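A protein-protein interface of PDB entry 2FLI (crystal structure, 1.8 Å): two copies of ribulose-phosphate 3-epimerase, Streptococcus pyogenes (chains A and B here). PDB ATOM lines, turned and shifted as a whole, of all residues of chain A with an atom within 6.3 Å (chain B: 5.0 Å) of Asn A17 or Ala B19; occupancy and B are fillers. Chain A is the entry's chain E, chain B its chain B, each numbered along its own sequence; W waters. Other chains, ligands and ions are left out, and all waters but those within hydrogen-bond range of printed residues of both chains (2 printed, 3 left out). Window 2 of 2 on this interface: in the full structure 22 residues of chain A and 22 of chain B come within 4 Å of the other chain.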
ATOM      1  N   ASP A  14     -18.412  29.927  31.236  1.00  0.00           N
ATOM      2  CA  ASP A  14     -19.093  30.579  30.117  1.00  0.00           C
ATOM      3  C   ASP A  14     -20.537  30.079  30.031  1.00  0.00           C
ATOM      4  O   ASP A  14     -20.809  29.011  29.479  1.00  0.00           O
ATOM      5  CB  ASP A  14     -18.336  30.281  28.816  1.00  0.00           C
ATOM      6  CG  ASP A  14     -19.032  30.821  27.584  1.00  0.00           C
ATOM      7  OD1 ASP A  14     -19.950  31.664  27.711  1.00  0.00           O
ATOM      8  OD2 ASP A  14     -18.646  30.407  26.471  1.00  0.00           O
ATOM      9  N   TYR A  15     -21.459  30.868  30.579  1.00  0.00           N
ATOM     10  CA  TYR A  15     -22.874  30.506  30.607  1.00  0.00           C
ATOM     11  C   TYR A  15     -23.504  30.161  29.264  1.00  0.00           C
ATOM     12  O   TYR A  15     -24.491  29.427  29.222  1.00  0.00           O
ATOM     13  CB  TYR A  15     -23.700  31.623  31.248  1.00  0.00           C
ATOM     14  CG  TYR A  15     -23.253  32.034  32.627  1.00  0.00           C
ATOM     15  CD1 TYR A  15     -22.564  31.152  33.457  1.00  0.00           C
ATOM     16  CD2 TYR A  15     -23.557  33.299  33.119  1.00  0.00           C
ATOM     17  CE1 TYR A  15     -22.191  31.524  34.746  1.00  0.00           C
ATOM     18  CE2 TYR A  15     -23.192  33.677  34.402  1.00  0.00           C
ATOM     19  CZ  TYR A  15     -22.510  32.788  35.210  1.00  0.00           C
ATOM     20  OH  TYR A  15     -22.152  33.177  36.480  1.00  0.00           O
ATOM     21  N   ALA A  16     -22.953  30.686  28.173  1.00  0.00           N
ATOM     22  CA  ALA A  16     -23.514  30.428  26.849  1.00  0.00           C
ATOM     23  C   ALA A  16     -23.119  29.061  26.295  1.00  0.00           C
ATOM     24  O   ALA A  16     -23.608  28.643  25.246  1.00  0.00           O
ATOM     25  CB  ALA A  16     -23.087  31.529  25.882  1.00  0.00           C
ATOM     26  N   ASN A  17     -22.239  28.365  27.007  1.00  0.00           N
ATOM     27  CA  ASN A  17     -21.781  27.050  26.577  1.00  0.00           C
ATOM     28  C   ASN A  17     -21.555  26.146  27.781  1.00  0.00           C
ATOM     29  O   ASN A  17     -20.442  25.662  27.997  1.00  0.00           O
ATOM     30  CB  ASN A  17     -20.470  27.177  25.789  1.00  0.00           C
ATOM     31  CG  ASN A  17     -20.673  27.761  24.403  1.00  0.00           C
ATOM     32  OD1 ASN A  17     -21.275  27.129  23.533  1.00  0.00           O
ATOM     33  ND2 ASN A  17     -20.172  28.972  24.191  1.00  0.00           N
ATOM     34  N   PHE A  18     -22.604  25.916  28.565  1.00  0.00           N
ATOM     35  CA  PHE A  18     -22.466  25.072  29.747  1.00  0.00           C
ATOM     36  C   PHE A  18     -21.935  23.685  29.418  1.00  0.00           C
ATOM     37  O   PHE A  18     -21.061  23.173  30.116  1.00  0.00           O
ATOM     38  CB  PHE A  18     -23.803  24.946  30.483  1.00  0.00           C
ATOM     39  CG  PHE A  18     -24.111  26.109  31.380  1.00  0.00           C
ATOM     40  CD1 PHE A  18     -23.193  26.516  32.341  1.00  0.00           C
ATOM     41  CD2 PHE A  18     -25.322  26.784  31.280  1.00  0.00           C
ATOM     42  CE1 PHE A  18     -23.473  27.578  33.192  1.00  0.00           C
ATOM     43  CE2 PHE A  18     -25.613  27.848  32.126  1.00  0.00           C
ATOM     44  CZ  PHE A  18     -24.687  28.246  33.082  1.00  0.00           C
ATOM     45  N   ALA A  19     -22.466  23.081  28.358  1.00  0.00           N
ATOM     46  CA  ALA A  19     -22.040  21.745  27.950  1.00  0.00           C
ATOM     47  C   ALA A  19     -20.532  21.639  27.710  1.00  0.00           C
ATOM     48  O   ALA A  19     -19.892  20.708  28.198  1.00  0.00           O
ATOM     49  CB  ALA A  19     -22.806  21.303  26.698  1.00  0.00           C
ATOM     50  N   SER A  20     -19.957  22.583  26.972  1.00  0.00           N
ATOM     51  CA  SER A  20     -18.518  22.523  26.716  1.00  0.00           C
ATOM     52  C   SER A  20     -17.697  22.855  27.963  1.00  0.00           C
ATOM     53  O   SER A  20     -16.565  22.396  28.112  1.00  0.00           O
ATOM     54  CB  SER A  20     -18.130  23.445  25.552  1.00  0.00           C
ATOM     55  OG  SER A  20     -18.474  24.793  25.794  1.00  0.00           O
ATOM     56  N   GLU A  21     -18.267  23.643  28.870  1.00  0.00           N
ATOM     57  CA  GLU A  21     -17.558  23.980  30.098  1.00  0.00           C
ATOM     58  C   GLU A  21     -17.529  22.751  30.995  1.00  0.00           C
ATOM     59  O   GLU A  21     -16.521  22.474  31.651  1.00  0.00           O
ATOM     60  CB  GLU A  21     -18.242  25.146  30.819  1.00  0.00           C
ATOM     61  CG  GLU A  21     -18.102  26.474  30.102  1.00  0.00           C
ATOM     62  CD  GLU A  21     -16.669  26.989  30.105  1.00  0.00           C
ATOM     63  OE1 GLU A  21     -16.400  27.992  30.802  1.00  0.00           O
ATOM     64  OE2 GLU A  21     -15.810  26.387  29.417  1.00  0.00           O
ATOM     65  N   LEU A  22     -18.640  22.013  31.015  1.00  0.00           N
ATOM     66  CA  LEU A  22     -18.740  20.808  31.828  1.00  0.00           C
ATOM     67  C   LEU A  22     -17.754  19.778  31.300  1.00  0.00           C
ATOM     68  O   LEU A  22     -17.158  19.020  32.068  1.00  0.00           O
ATOM     69  CB  LEU A  22     -20.166  20.243  31.784  1.00  0.00           C
ATOM     70  CG  LEU A  22     -21.210  21.063  32.550  1.00  0.00           C
ATOM     71  CD1 LEU A  22     -22.619  20.561  32.266  1.00  0.00           C
ATOM     72  CD2 LEU A  22     -20.893  20.984  34.031  1.00  0.00           C
ATOM     73  N   ALA B  16     -28.072  24.191  28.018  1.00  0.00           N
ATOM     74  CA  ALA B  16     -26.658  23.812  28.043  1.00  0.00           C
ATOM     75  C   ALA B  16     -25.884  24.302  26.808  1.00  0.00           C
ATOM     76  O   ALA B  16     -24.662  24.138  26.718  1.00  0.00           O
ATOM     77  CB  ALA B  16     -26.535  22.302  28.174  1.00  0.00           C
ATOM     78  N   ASN B  17     -26.600  24.911  25.868  1.00  0.00           N
ATOM     79  CA  ASN B  17     -26.008  25.422  24.637  1.00  0.00           C
ATOM     80  C   ASN B  17     -26.715  26.695  24.188  1.00  0.00           C
ATOM     81  O   ASN B  17     -27.279  26.748  23.093  1.00  0.00           O
ATOM     82  CB  ASN B  17     -26.115  24.379  23.525  1.00  0.00           C
ATOM     83  CG  ASN B  17     -25.193  23.195  23.744  1.00  0.00           C
ATOM     84  OD1 ASN B  17     -23.973  23.342  23.740  1.00  0.00           O
ATOM     85  ND2 ASN B  17     -25.773  22.016  23.934  1.00  0.00           N
ATOM     86  N   PHE B  18     -26.692  27.723  25.025  1.00  0.00           N
ATOM     87  CA  PHE B  18     -27.354  28.966  24.660  1.00  0.00           C
ATOM     88  C   PHE B  18     -26.797  29.539  23.358  1.00  0.00           C
ATOM     89  O   PHE B  18     -27.550  30.045  22.521  1.00  0.00           O
ATOM     90  CB  PHE B  18     -27.222  29.994  25.791  1.00  0.00           C
ATOM     91  CG  PHE B  18     -28.197  29.779  26.933  1.00  0.00           C
ATOM     92  CD1 PHE B  18     -29.570  29.709  26.693  1.00  0.00           C
ATOM     93  CD2 PHE B  18     -27.749  29.683  28.243  1.00  0.00           C
ATOM     94  CE1 PHE B  18     -30.479  29.550  27.745  1.00  0.00           C
ATOM     95  CE2 PHE B  18     -28.648  29.525  29.300  1.00  0.00           C
ATOM     96  CZ  PHE B  18     -30.013  29.459  29.050  1.00  0.00           C
ATOM     97  N   ALA B  19     -25.481  29.450  23.188  1.00  0.00           N
ATOM     98  CA  ALA B  19     -24.823  29.969  21.992  1.00  0.00           C
ATOM     99  C   ALA B  19     -25.394  29.377  20.700  1.00  0.00           C
ATOM    100  O   ALA B  19     -25.880  30.109  19.838  1.00  0.00           O
ATOM    101  CB  ALA B  19     -23.323  29.711  22.069  1.00  0.00           C
ATOM    102  N   SER B  20     -25.341  28.058  20.559  1.00  0.00           N
ATOM    103  CA  SER B  20     -25.864  27.426  19.349  1.00  0.00           C
ATOM    104  C   SER B  20     -27.364  27.664  19.201  1.00  0.00           C
ATOM    105  O   SER B  20     -27.863  27.835  18.088  1.00  0.00           O
ATOM    106  CB  SER B  20     -25.567  25.924  19.350  1.00  0.00           C
ATOM    107  OG  SER B  20     -26.088  25.287  20.498  1.00  0.00           O
ATOM    108  N   GLU B  21     -28.082  27.689  20.320  1.00  0.00           N
ATOM    109  CA  GLU B  21     -29.521  27.922  20.273  1.00  0.00           C
ATOM    110  C   GLU B  21     -29.808  29.328  19.745  1.00  0.00           C
ATOM    111  O   GLU B  21     -30.751  29.528  18.978  1.00  0.00           O
ATOM    112  CB  GLU B  21     -30.141  27.726  21.663  1.00  0.00           C
ATOM    113  CG  GLU B  21     -30.153  26.271  22.122  1.00  0.00           C
ATOM    114  CD  GLU B  21     -31.138  25.414  21.335  1.00  0.00           C
ATOM    115  OE1 GLU B  21     -32.244  25.144  21.846  1.00  0.00           O
ATOM    116  OE2 GLU B  21     -30.812  25.020  20.198  1.00  0.00           O
ATOM    117  N   LEU B  22     -28.992  30.295  20.157  1.00  0.00           N
ATOM    118  CA  LEU B  22     -29.153  31.673  19.701  1.00  0.00           C
ATOM    119  C   LEU B  22     -28.809  31.745  18.215  1.00  0.00           C
ATOM    120  O   LEU B  22     -29.426  32.497  17.458  1.00  0.00           O
ATOM    121  CB  LEU B  22     -28.239  32.611  20.495  1.00  0.00           C
ATOM    122  CG  LEU B  22     -28.684  32.932  21.924  1.00  0.00           C
ATOM    123  CD1 LEU B  22     -27.515  33.501  22.711  1.00  0.00           C
ATOM    124  CD2 LEU B  22     -29.843  33.919  21.890  1.00  0.00           C
ATOM    125  N   ALA B  23     -27.818  30.956  17.809  1.00  0.00           N
ATOM    126  CA  ALA B  23     -27.400  30.913  16.410  1.00  0.00           C
ATOM    127  C   ALA B  23     -28.531  30.337  15.559  1.00  0.00           C
ATOM    128  O   ALA B  23     -28.747  30.766  14.426  1.00  0.00           O
ATOM    129  CB  ALA B  23     -26.136  30.065  16.259  1.00  0.00           C
ATOM    130  N   HIS B  59     -23.394  36.464  21.581  1.00  0.00           N
ATOM    131  CA  HIS B  59     -23.656  35.397  20.624  1.00  0.00           C
ATOM    132  C   HIS B  59     -24.932  35.668  19.844  1.00  0.00           C
ATOM    133  O   HIS B  59     -25.506  34.764  19.242  1.00  0.00           O
ATOM    134  CB  HIS B  59     -23.769  34.060  21.354  1.00  0.00           C
ATOM    135  CG  HIS B  59     -22.529  33.678  22.098  1.00  0.00           C
ATOM    136  ND1 HIS B  59     -21.388  33.236  21.467  1.00  0.00           N
ATOM    137  CD2 HIS B  59     -22.246  33.695  23.421  1.00  0.00           C
ATOM    138  CE1 HIS B  59     -20.453  32.997  22.370  1.00  0.00           C
ATOM    139  NE2 HIS B  59     -20.948  33.267  23.564  1.00  0.00           N
HETATM  140  O   HOH W   1     -18.280  32.421  24.719  1.00  0.00           O
HETATM  141  O   HOH W   2     -20.393  33.944  26.228  1.00  0.00           O
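O of Ala B16 sits at hydrogen-bond distance from N of Ala A19.
The backbone NH (N) of Ala B19 sits at hydrogen-bond distance from the backbone carbonyl oxygen (O) of Ala A16 (2.9 Å).
The backbone NH (N) of Phe A18 is in hydrogen-bond range of the backbone carbonyl oxygen (O) of Ala B16, 3.3 Å away.
O of Ala A16 sits at hydrogen-bond distance from N of Phe B18 (3.2 Å).
ND2 of Asn A17 lies within hydrogen-bond range of OD2 of Asp A14, 3.1 Å away.
OG of Ser A20 is in hydrogen-bond range of O of Asn A17 (3.1 Å).
The backbone carbonyl oxygen (O) of Asn B17 sits close to the side-chain hydroxyl (OG) of Ser B20, 3.2 Å away.
The side-chain carboxylate of Asp A14 lies close to the backbone NH of Ala A16.
Among the printed residues, merely in contact across the chains: Tyr A15 with Phe B18 (3.4 Å), Ala A16 with Asn B17 (3.8 Å), Ala A16 with His B59 (3.4 Å), Asn A17 with Ala B16 (3.8 Å), Asn A17 with Ala B19 (3.6 Å) and Ala A19 with Asn B17 (3.8 Å).
Asn A17 touches two residues of chain B.
Of chain A, only Ala A16 and Asn A17 come within 4 Å of Ala B19.
Of the printed residues of chain A, Ala B16 touches Asn A17 (3.8 Å), Phe A18 (3.3 Å) and Ala A19 (2.9 Å).
Of the printed residues of chain A, Asn B17 touches Ala A16 and Ala A19.
Printed residues of chain A within 4 Å of His B59: Ala A16.
The nearest residue of chain B that does not touch Asn A17 is His B59 (4.4 Å).
Among the printed residues, 10 pairs touch across the chains.
Among the printed residues, no Asp or Glu carboxylate lies within 4 Å of a Lys or Arg side-chain nitrogen of the other chain.
Ala A16 touches Asn B17, and with the chains exchanged Asn A17 touches Ala B16.
Ala A16 touches Phe B18, and with the chains exchanged Phe A18 touches Ala B16.
Ala A16 touches Ala B19, and with the chains exchanged Ala A19 touches Ala B16.
Asn A17 touches Ala B19, and with the chains exchanged Ala A19 touches Asn B17.
Positions printed for both chains: 16, 17, 18, 19, 20, 21 and 22.
Of the 10 pairs that touch across the chains among the printed residues, 8 have their exchanged pair printed and touching as well.
Water W1 lies within hydrogen-bond range of OD2 of Asp A14 (2.7 Å) and NE2 of His B59 (3.0 Å).
Water W2 lies within hydrogen-bond range of OD1 of Asp A14 (2.8 Å) and NE2 of His B59 (2.8 Å).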
